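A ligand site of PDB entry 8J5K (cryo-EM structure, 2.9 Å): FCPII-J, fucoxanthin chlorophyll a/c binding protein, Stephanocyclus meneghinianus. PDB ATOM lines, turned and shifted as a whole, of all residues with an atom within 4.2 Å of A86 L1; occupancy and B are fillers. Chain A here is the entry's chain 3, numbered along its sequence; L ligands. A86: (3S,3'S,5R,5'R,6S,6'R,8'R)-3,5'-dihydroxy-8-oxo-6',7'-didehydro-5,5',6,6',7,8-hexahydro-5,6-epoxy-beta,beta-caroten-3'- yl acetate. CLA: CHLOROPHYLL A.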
ATOM      1  N   MET A  42      23.217 -19.354  23.444  1.00  0.00           N
ATOM      2  CA  MET A  42      23.033 -17.964  23.054  1.00  0.00           C
ATOM      3  C   MET A  42      21.718 -17.440  23.602  1.00  0.00           C
ATOM      4  O   MET A  42      21.642 -16.340  24.180  1.00  0.00           O
ATOM      5  CB  MET A  42      23.020 -17.839  21.537  1.00  0.00           C
ATOM      6  CG  MET A  42      24.340 -17.542  20.883  1.00  0.00           C
ATOM      7  N   VAL A  45      21.986 -16.730  27.360  1.00  0.00           N
ATOM      8  CA  VAL A  45      22.593 -15.445  27.736  1.00  0.00           C
ATOM      9  C   VAL A  45      21.601 -14.310  27.542  1.00  0.00           C
ATOM     10  O   VAL A  45      21.414 -13.440  28.417  1.00  0.00           O
ATOM     11  CB  VAL A  45      23.884 -15.204  26.928  1.00  0.00           C
ATOM     12  CG1 VAL A  45      24.297 -13.744  27.005  1.00  0.00           C
ATOM     13  CG2 VAL A  45      24.989 -16.076  27.446  1.00  0.00           C
ATOM     14  N   LEU A  46      20.944 -14.296  26.372  1.00  0.00           N
ATOM     15  CA  LEU A  46      19.915 -13.287  26.132  1.00  0.00           C
ATOM     16  C   LEU A  46      18.826 -13.364  27.188  1.00  0.00           C
ATOM     17  O   LEU A  46      18.313 -12.335  27.648  1.00  0.00           O
ATOM     18  CB  LEU A  46      19.296 -13.495  24.754  1.00  0.00           C
ATOM     19  CG  LEU A  46      20.213 -13.290  23.561  1.00  0.00           C
ATOM     20  CD1 LEU A  46      19.453 -13.678  22.317  1.00  0.00           C
ATOM     21  CD2 LEU A  46      20.660 -11.856  23.494  1.00  0.00           C
ATOM     22  N   VAL A  49      20.111 -11.668  30.610  1.00  0.00           N
ATOM     23  CA  VAL A  49      20.177 -10.205  30.630  1.00  0.00           C
ATOM     24  C   VAL A  49      18.770  -9.593  30.579  1.00  0.00           C
ATOM     25  O   VAL A  49      18.504  -8.590  31.253  1.00  0.00           O
ATOM     26  CB  VAL A  49      21.094  -9.699  29.501  1.00  0.00           C
ATOM     27  CG1 VAL A  49      21.083  -8.208  29.432  1.00  0.00           C
ATOM     28  CG2 VAL A  49      22.500 -10.166  29.753  1.00  0.00           C
ATOM     29  N   SER A 103      10.359 -19.100  12.589  1.00  0.00           N
ATOM     30  CA  SER A 103      10.682 -19.187  11.166  1.00  0.00           C
ATOM     31  C   SER A 103      10.493 -20.623  10.670  1.00  0.00           C
ATOM     32  O   SER A 103      11.475 -21.304  10.360  1.00  0.00           O
ATOM     33  CB  SER A 103      12.108 -18.698  10.893  1.00  0.00           C
ATOM     34  OG  SER A 103      13.062 -19.610  11.386  1.00  0.00           O
ATOM     35  N   THR A 105       9.504 -21.778   7.858  1.00  0.00           N
ATOM     36  CA  THR A 105      10.196 -21.811   6.583  1.00  0.00           C
ATOM     37  C   THR A 105      10.846 -20.457   6.357  1.00  0.00           C
ATOM     38  O   THR A 105      10.681 -19.522   7.148  1.00  0.00           O
ATOM     39  CB  THR A 105       9.246 -22.155   5.430  1.00  0.00           C
ATOM     40  N   GLY A 106      11.617 -20.366   5.279  1.00  0.00           N
ATOM     41  CA  GLY A 106      12.233 -19.110   4.892  1.00  0.00           C
ATOM     42  C   GLY A 106      13.663 -18.982   5.400  1.00  0.00           C
ATOM     43  O   GLY A 106      13.873 -18.803   6.600  1.00  0.00           O
ATOM     44  N   HIS A 125      29.998 -18.169  17.201  1.00  0.00           N
ATOM     45  CA  HIS A 125      29.237 -17.420  18.192  1.00  0.00           C
ATOM     46  C   HIS A 125      28.582 -18.338  19.215  1.00  0.00           C
ATOM     47  O   HIS A 125      28.601 -18.054  20.419  1.00  0.00           O
ATOM     48  CB  HIS A 125      28.173 -16.578  17.491  1.00  0.00           C
ATOM     49  CG  HIS A 125      28.698 -15.267  17.020  1.00  0.00           C
ATOM     50  ND1 HIS A 125      29.133 -15.062  15.734  1.00  0.00           N
ATOM     51  CD2 HIS A 125      28.909 -14.103  17.688  1.00  0.00           C
ATOM     52  CE1 HIS A 125      29.556 -13.813  15.608  1.00  0.00           C
ATOM     53  NE2 HIS A 125      29.436 -13.220  16.787  1.00  0.00           N
ATOM     54  N   LEU A 128      31.057 -19.664  21.654  1.00  0.00           N
ATOM     55  CA  LEU A 128      31.370 -18.661  22.664  1.00  0.00           C
ATOM     56  C   LEU A 128      30.264 -18.560  23.710  1.00  0.00           C
ATOM     57  O   LEU A 128      30.524 -18.422  24.912  1.00  0.00           O
ATOM     58  CB  LEU A 128      31.595 -17.314  21.989  1.00  0.00           C
ATOM     59  CG  LEU A 128      32.231 -16.234  22.859  1.00  0.00           C
ATOM     60  CD1 LEU A 128      33.445 -16.791  23.563  1.00  0.00           C
ATOM     61  CD2 LEU A 128      32.602 -15.043  22.001  1.00  0.00           C
ATOM     62  N   ALA A 132      29.955 -18.479  27.855  1.00  0.00           N
ATOM     63  CA  ALA A 132      29.275 -17.392  28.565  1.00  0.00           C
ATOM     64  C   ALA A 132      28.236 -17.939  29.541  1.00  0.00           C
ATOM     65  O   ALA A 132      28.162 -17.492  30.702  1.00  0.00           O
ATOM     66  CB  ALA A 132      28.636 -16.450  27.557  1.00  0.00           C
ATOM     67  N   GLU A 135      30.109 -19.289  32.664  1.00  0.00           N
ATOM     68  CA  GLU A 135      30.529 -18.348  33.679  1.00  0.00           C
ATOM     69  C   GLU A 135      29.349 -17.850  34.460  1.00  0.00           C
ATOM     70  O   GLU A 135      29.414 -17.701  35.675  1.00  0.00           O
ATOM     71  CB  GLU A 135      31.259 -17.161  33.065  1.00  0.00           C
ATOM     72  CG  GLU A 135      31.575 -16.032  34.033  1.00  0.00           C
ATOM     73  CD  GLU A 135      32.682 -16.393  35.005  1.00  0.00           C
ATOM     74  OE1 GLU A 135      33.129 -17.548  35.014  1.00  0.00           O
ATOM     75  OE2 GLU A 135      33.101 -15.489  35.768  1.00  0.00           O
ATOM     76  N   LEU A 136      28.258 -17.576  33.755  1.00  0.00           N
ATOM     77  CA  LEU A 136      27.092 -17.021  34.420  1.00  0.00           C
ATOM     78  C   LEU A 136      26.609 -17.983  35.480  1.00  0.00           C
ATOM     79  O   LEU A 136      26.436 -17.605  36.629  1.00  0.00           O
ATOM     80  CB  LEU A 136      26.004 -16.722  33.406  1.00  0.00           C
ATOM     81  CG  LEU A 136      26.363 -15.604  32.431  1.00  0.00           C
ATOM     82  CD1 LEU A 136      25.518 -15.649  31.169  1.00  0.00           C
ATOM     83  CD2 LEU A 136      26.271 -14.249  33.115  1.00  0.00           C
ATOM     84  N   ILE A 156      24.954  -9.972  37.220  1.00  0.00           N
ATOM     85  CA  ILE A 156      25.699  -9.756  35.983  1.00  0.00           C
ATOM     86  C   ILE A 156      26.896  -8.910  36.400  1.00  0.00           C
ATOM     87  O   ILE A 156      26.754  -7.725  36.733  1.00  0.00           O
ATOM     88  CB  ILE A 156      24.839  -9.085  34.917  1.00  0.00           C
ATOM     89  CG1 ILE A 156      23.693 -10.004  34.537  1.00  0.00           C
ATOM     90  CG2 ILE A 156      25.574  -8.952  33.635  1.00  0.00           C
ATOM     91  CD1 ILE A 156      22.505  -9.823  35.356  1.00  0.00           C
ATOM     92  N   THR A 157      28.075  -9.530  36.479  1.00  0.00           N
ATOM     93  CA  THR A 157      29.237  -8.850  37.017  1.00  0.00           C
ATOM     94  C   THR A 157      29.676  -7.719  36.097  1.00  0.00           C
ATOM     95  O   THR A 157      29.852  -6.578  36.546  1.00  0.00           O
ATOM     96  CB  THR A 157      30.381  -9.849  37.248  1.00  0.00           C
ATOM     97  OG1 THR A 157      29.948 -10.843  38.177  1.00  0.00           O
ATOM     98  CG2 THR A 157      31.582  -9.130  37.821  1.00  0.00           C
ATOM     99  N   GLY A 158      29.823  -8.014  34.813  1.00  0.00           N
ATOM    100  CA  GLY A 158      29.907  -6.963  33.832  1.00  0.00           C
ATOM    101  C   GLY A 158      28.540  -6.327  33.643  1.00  0.00           C
ATOM    102  O   GLY A 158      27.590  -6.613  34.367  1.00  0.00           O
ATOM    103  N   LEU A 159      28.449  -5.466  32.636  1.00  0.00           N
ATOM    104  CA  LEU A 159      27.276  -4.626  32.414  1.00  0.00           C
ATOM    105  C   LEU A 159      26.799  -3.979  33.715  1.00  0.00           C
ATOM    106  O   LEU A 159      25.667  -4.202  34.142  1.00  0.00           O
ATOM    107  CB  LEU A 159      26.156  -5.431  31.773  1.00  0.00           C
ATOM    108  CG  LEU A 159      26.469  -6.165  30.470  1.00  0.00           C
ATOM    109  CD1 LEU A 159      25.313  -7.049  30.054  1.00  0.00           C
ATOM    110  CD2 LEU A 159      26.755  -5.161  29.389  1.00  0.00           C
HETATM  111  C   A86 L   1      20.802 -14.014  18.895  1.00  0.00           C
HETATM  112  O   A86 L   1      30.135 -11.841  27.509  1.00  0.00           O
HETATM  113  C1  A86 L   1      21.963 -14.431  18.042  1.00  0.00           C
HETATM  114  C10 A86 L   1      27.913 -13.101  25.379  1.00  0.00           C
HETATM  115  C11 A86 L   1      29.065 -13.186  26.038  1.00  0.00           C
HETATM  116  C12 A86 L   1      30.261 -13.836  25.418  1.00  0.00           C
HETATM  117  C13 A86 L   1      29.195 -12.578  27.346  1.00  0.00           C
HETATM  118  C14 A86 L   1      28.234 -12.852  28.475  1.00  0.00           C
HETATM  119  C15 A86 L   1      28.668 -12.073  29.733  1.00  0.00           C
HETATM  120  C16 A86 L   1      28.099 -10.611  29.857  1.00  0.00           C
HETATM  121  C17 A86 L   1      28.670  -9.864  31.042  1.00  0.00           C
HETATM  122  C18 A86 L   1      28.363 -10.654  32.283  1.00  0.00           C
HETATM  123  C19 A86 L   1      29.138 -11.925  32.243  1.00  0.00           C
HETATM  124  C2  A86 L   1      23.210 -14.459  18.519  1.00  0.00           C
HETATM  125  C20 A86 L   1      29.018 -12.812  31.055  1.00  0.00           C
HETATM  126  C21 A86 L   1      29.697 -14.152  31.085  1.00  0.00           C
HETATM  127  C22 A86 L   1      26.590 -10.717  30.027  1.00  0.00           C
HETATM  128  C23 A86 L   1      28.240  -9.650  28.669  1.00  0.00           C
HETATM  129  C24 A86 L   1      21.783 -14.850  16.646  1.00  0.00           C
HETATM  130  C25 A86 L   1      20.602 -14.946  16.060  1.00  0.00           C
HETATM  131  C26 A86 L   1      20.621 -15.387  14.663  1.00  0.00           C
HETATM  132  C27 A86 L   1      19.482 -15.533  13.998  1.00  0.00           C
HETATM  133  C28 A86 L   1      18.201 -15.329  14.735  1.00  0.00           C
HETATM  134  C29 A86 L   1      19.467 -15.983  12.595  1.00  0.00           C
HETATM  135  C3  A86 L   1      23.511 -14.087  19.882  1.00  0.00           C
HETATM  136  C30 A86 L   1      18.340 -15.906  12.055  1.00  0.00           C
HETATM  137  C31 A86 L   1      17.228 -15.824  11.507  1.00  0.00           C
HETATM  138  C32 A86 L   1      16.874 -14.435  10.993  1.00  0.00           C
HETATM  139  C33 A86 L   1      15.402 -14.181  11.116  1.00  0.00           C
HETATM  140  C34 A86 L   1      14.688 -15.221  10.268  1.00  0.00           C
HETATM  141  C35 A86 L   1      14.992 -16.578  10.861  1.00  0.00           C
HETATM  142  C36 A86 L   1      16.454 -16.984  10.965  1.00  0.00           C
HETATM  143  C37 A86 L   1      16.482 -18.077  12.012  1.00  0.00           C
HETATM  144  C38 A86 L   1      12.373 -15.659   9.435  1.00  0.00           C
HETATM  145  C39 A86 L   1      12.858 -16.276   8.154  1.00  0.00           C
HETATM  146  C4  A86 L   1      24.769 -14.195  20.277  1.00  0.00           C
HETATM  147  C40 A86 L   1      17.544 -13.337  11.796  1.00  0.00           C
HETATM  148  C41 A86 L   1      17.361 -14.296   9.560  1.00  0.00           C
HETATM  149  C5  A86 L   1      25.101 -13.824  21.645  1.00  0.00           C
HETATM  150  C6  A86 L   1      26.342 -13.957  22.121  1.00  0.00           C
HETATM  151  C7  A86 L   1      27.451 -14.483  21.268  1.00  0.00           C
HETATM  152  C8  A86 L   1      26.593 -13.512  23.487  1.00  0.00           C
HETATM  153  C9  A86 L   1      27.773 -13.641  24.043  1.00  0.00           C
HETATM  154  O1  A86 L   1      27.768 -12.947  30.419  1.00  0.00           O
HETATM  155  O2  A86 L   1      28.773  -9.942  33.441  1.00  0.00           O
HETATM  156  O3  A86 L   1      16.955 -17.499   9.729  1.00  0.00           O
HETATM  157  O4  A86 L   1      13.282 -14.971  10.333  1.00  0.00           O
HETATM  158  O5  A86 L   1      11.183 -15.553   9.657  1.00  0.00           O
HETATM  159 MG   CLA L   2      21.451 -18.902  12.623  1.00  0.00          MG
HETATM  160  CHA CLA L   2      19.739 -20.335   9.984  1.00  0.00           C
HETATM  161  CHB CLA L   2      23.797 -17.720  10.510  1.00  0.00           C
HETATM  162  CHC CLA L   2      23.114 -17.590  15.326  1.00  0.00           C
HETATM  163  CHD CLA L   2      18.797 -19.828  14.736  1.00  0.00           C
HETATM  164  NA  CLA L   2      21.732 -19.071  10.576  1.00  0.00           N
HETATM  165  C1A CLA L   2      20.900 -19.692   9.646  1.00  0.00           C
HETATM  166  C2A CLA L   2      21.480 -19.556   8.232  1.00  0.00           C
HETATM  167  C3A CLA L   2      22.808 -18.817   8.469  1.00  0.00           C
HETATM  168  C4A CLA L   2      22.799 -18.495   9.961  1.00  0.00           C
HETATM  169  CMA CLA L   2      23.956 -19.712   8.087  1.00  0.00           C
HETATM  170  CAA CLA L   2      20.608 -18.695   7.340  1.00  0.00           C
HETATM  171  NB  CLA L   2      23.151 -17.866  12.874  1.00  0.00           N
HETATM  172  C1B CLA L   2      23.942 -17.384  11.876  1.00  0.00           C
HETATM  173  C2B CLA L   2      24.995 -16.501  12.457  1.00  0.00           C
HETATM  174  C3B CLA L   2      24.792 -16.483  13.817  1.00  0.00           C
HETATM  175  C4B CLA L   2      23.638 -17.375  14.097  1.00  0.00           C
HETATM  176  CMB CLA L   2      26.019 -15.815  11.690  1.00  0.00           C
HETATM  177  CAB CLA L   2      25.521 -15.830  14.867  1.00  0.00           C
HETATM  178  CBB CLA L   2      25.746 -14.522  14.993  1.00  0.00           C
HETATM  179  NC  CLA L   2      21.039 -18.769  14.659  1.00  0.00           N
HETATM  180  C1C CLA L   2      21.872 -18.234  15.587  1.00  0.00           C
HETATM  181  C2C CLA L   2      21.289 -18.403  16.912  1.00  0.00           C
HETATM  182  C3C CLA L   2      20.004 -18.923  16.703  1.00  0.00           C
HETATM  183  C4C CLA L   2      19.870 -19.146  15.287  1.00  0.00           C
HETATM  184  CMC CLA L   2      21.939 -18.017  18.156  1.00  0.00           C
HETATM  185  CAC CLA L   2      18.962 -19.277  17.671  1.00  0.00           C
HETATM  186  CBC CLA L   2      17.785 -18.336  17.634  1.00  0.00           C
HETATM  187  ND  CLA L   2      19.719 -19.925  12.488  1.00  0.00           N
HETATM  188  C1D CLA L   2      18.741 -20.260  13.446  1.00  0.00           C
HETATM  189  C2D CLA L   2      17.659 -21.048  12.811  1.00  0.00           C
HETATM  190  C3D CLA L   2      18.018 -21.125  11.486  1.00  0.00           C
HETATM  191  C4D CLA L   2      19.285 -20.381  11.333  1.00  0.00           C
HETATM  192  CMD CLA L   2      16.511 -21.613  13.512  1.00  0.00           C
HETATM  193  CAD CLA L   2      17.638 -21.616  10.180  1.00  0.00           C
HETATM  194  OBD CLA L   2      16.666 -22.280   9.841  1.00  0.00           O
HETATM  195  CBD CLA L   2      18.722 -21.107   9.186  1.00  0.00           C
HETATM  196  CGD CLA L   2      19.367 -22.256   8.476  1.00  0.00           C
HETATM  197  O1D CLA L   2      20.203 -23.038   8.934  1.00  0.00           O
HETATM  198  O2D CLA L   2      18.945 -22.409   7.192  1.00  0.00           O
HETATM  199 MG   CLA L   3      29.347 -10.400  16.334  1.00  0.00          MG
HETATM  200  CHA CLA L   3      30.412 -10.518  13.032  1.00  0.00           C
HETATM  201  CHB CLA L   3      26.118 -10.408  15.286  1.00  0.00           C
HETATM  202  CHC CLA L   3      28.340 -10.519  19.608  1.00  0.00           C
HETATM  203  CHD CLA L   3      32.723 -10.556  17.375  1.00  0.00           C
HETATM  204  NA  CLA L   3      28.440 -10.401  14.453  1.00  0.00           N
HETATM  205  C1A CLA L   3      29.047 -10.476  13.196  1.00  0.00           C
HETATM  206  C2A CLA L   3      27.991 -10.501  12.075  1.00  0.00           C
HETATM  207  C3A CLA L   3      26.663 -10.375  12.842  1.00  0.00           C
HETATM  208  C4A CLA L   3      27.086 -10.401  14.305  1.00  0.00           C
HETATM  209  CMA CLA L   3      25.919  -9.113  12.490  1.00  0.00           C
HETATM  210  CAA CLA L   3      27.979 -11.807  11.305  1.00  0.00           C
HETATM  211  NB  CLA L   3      27.568 -10.463  17.277  1.00  0.00           N
HETATM  212  C1B CLA L   3      26.368 -10.423  16.664  1.00  0.00           C
HETATM  213  C2B CLA L   3      25.289 -10.355  17.678  1.00  0.00           C
HETATM  214  C3B CLA L   3      25.881 -10.385  18.919  1.00  0.00           C
HETATM  215  C4B CLA L   3      27.354 -10.450  18.676  1.00  0.00           C
HETATM  216  CMB CLA L   3      23.869 -10.302  17.329  1.00  0.00           C
HETATM  217  CAB CLA L   3      25.169 -10.356  20.181  1.00  0.00           C
HETATM  218  CBB CLA L   3      25.610 -10.522  21.426  1.00  0.00           C
HETATM  219  NC  CLA L   3      30.360 -10.473  18.151  1.00  0.00           N
HETATM  220  C1C CLA L   3      29.747 -10.526  19.367  1.00  0.00           C
HETATM  221  C2C CLA L   3      30.740 -10.616  20.425  1.00  0.00           C
HETATM  222  C3C CLA L   3      31.992 -10.625  19.807  1.00  0.00           C
HETATM  223  C4C CLA L   3      31.737 -10.545  18.371  1.00  0.00           C
HETATM  224  CMC CLA L   3      30.439 -10.698  21.858  1.00  0.00           C
HETATM  225  ND  CLA L   3      31.171 -10.396  15.477  1.00  0.00           N
HETATM  226  C1D CLA L   3      32.482 -10.501  16.025  1.00  0.00           C
HETATM  227  C2D CLA L   3      33.458 -10.521  14.916  1.00  0.00           C
HETATM  228  C3D CLA L   3      32.722 -10.508  13.751  1.00  0.00           C
HETATM  229  C4D CLA L   3      31.301 -10.472  14.150  1.00  0.00           C
HETATM  230  CMD CLA L   3      34.908 -10.567  15.096  1.00  0.00           C
HETATM  231  CAD CLA L   3      32.771 -10.523  12.309  1.00  0.00           C
HETATM  232  OBD CLA L   3      33.734 -10.510  11.552  1.00  0.00           O
HETATM  233  CBD CLA L   3      31.287 -10.587  11.806  1.00  0.00           C
HETATM  234 MG   CLA L   4      31.786  -4.989  31.289  1.00  0.00          MG
HETATM  235  CHA CLA L   4      33.551  -7.209  33.255  1.00  0.00           C
HETATM  236  CHB CLA L   4      32.453  -2.503  33.497  1.00  0.00           C
HETATM  237  CHC CLA L   4      30.127  -2.800  29.244  1.00  0.00           C
HETATM  238  CHD CLA L   4      31.179  -7.587  28.970  1.00  0.00           C
HETATM  239  NA  CLA L   4      32.802  -4.913  33.103  1.00  0.00           N
HETATM  240  C1A CLA L   4      33.488  -5.944  33.760  1.00  0.00           C
HETATM  241  C2A CLA L   4      34.089  -5.441  35.076  1.00  0.00           C
HETATM  242  C3A CLA L   4      33.584  -3.994  35.182  1.00  0.00           C
HETATM  243  C4A CLA L   4      32.893  -3.766  33.842  1.00  0.00           C
HETATM  244  CMA CLA L   4      32.628  -3.809  36.331  1.00  0.00           C
HETATM  245  CAA CLA L   4      35.605  -5.453  35.071  1.00  0.00           C
HETATM  246  CBA CLA L   4      36.172  -4.978  33.745  1.00  0.00           C
HETATM  247  NB  CLA L   4      31.348  -3.033  31.371  1.00  0.00           N
HETATM  248  C1B CLA L   4      31.789  -2.165  32.316  1.00  0.00           C
HETATM  249  C2B CLA L   4      31.400  -0.782  31.949  1.00  0.00           C
HETATM  250  C3B CLA L   4      30.739  -0.853  30.745  1.00  0.00           C
HETATM  251  C4B CLA L   4      30.685  -2.296  30.368  1.00  0.00           C
HETATM  252  CMB CLA L   4      31.716   0.377  32.771  1.00  0.00           C
HETATM  253  CAB CLA L   4      30.153   0.191  29.963  1.00  0.00           C
HETATM  254  CBB CLA L   4      30.493   0.507  28.700  1.00  0.00           C
HETATM  255  NC  CLA L   4      30.801  -5.174  29.451  1.00  0.00           N
HETATM  256  C1C CLA L   4      30.186  -4.149  28.808  1.00  0.00           C
HETATM  257  C2C CLA L   4      29.588  -4.630  27.562  1.00  0.00           C
HETATM  258  C3C CLA L   4      29.897  -5.981  27.471  1.00  0.00           C
HETATM  259  C4C CLA L   4      30.667  -6.315  28.672  1.00  0.00           C
HETATM  260  CMC CLA L   4      28.834  -3.804  26.625  1.00  0.00           C
HETATM  261  CAC CLA L   4      29.517  -6.906  26.400  1.00  0.00           C
HETATM  262  CBC CLA L   4      30.645  -7.184  25.446  1.00  0.00           C
HETATM  263  ND  CLA L   4      32.190  -6.946  31.119  1.00  0.00           N
HETATM  264  C1D CLA L   4      31.900  -7.893  30.098  1.00  0.00           C
HETATM  265  C2D CLA L   4      32.469  -9.195  30.482  1.00  0.00           C
HETATM  266  C3D CLA L   4      33.112  -9.000  31.681  1.00  0.00           C
HETATM  267  C4D CLA L   4      32.915  -7.579  32.022  1.00  0.00           C
HETATM  268  CMD CLA L   4      32.340 -10.403  29.669  1.00  0.00           C
HETATM  269  CAD CLA L   4      33.900  -9.601  32.747  1.00  0.00           C
HETATM  270  OBD CLA L   4      34.266 -10.755  32.873  1.00  0.00           O
HETATM  271  CBD CLA L   4      34.216  -8.470  33.766  1.00  0.00           C
HETATM  272  CGD CLA L   4      33.731  -8.782  35.143  1.00  0.00           C
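Merely in contact with A86 L1: Gly 106 (3.1 Å), Leu 136 (3.3 Å), Ile 156 (3.4 Å), Ser 103 (3.4 Å), Met 42 (3.4 Å), Ala 132 (3.6 Å), Leu 46 (3.7 Å), His 125 (3.8 Å), Leu 159 (3.9 Å) and Glu 135 (3.9 Å). Hydrophobic or aromatic side chains that line A86 L1: Met 42, Leu 46, His 125, Ala 132, Leu 136, Ile 156 and Leu 159.
The backbone NH (N) of Thr 157 sits at hydrogen-bond distance from an oxygen (O2) of A86 L1. An oxygen (O2) of A86 L1 is in hydrogen-bond range of the backbone NH (N) of Gly 158, at 2.6 Å.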
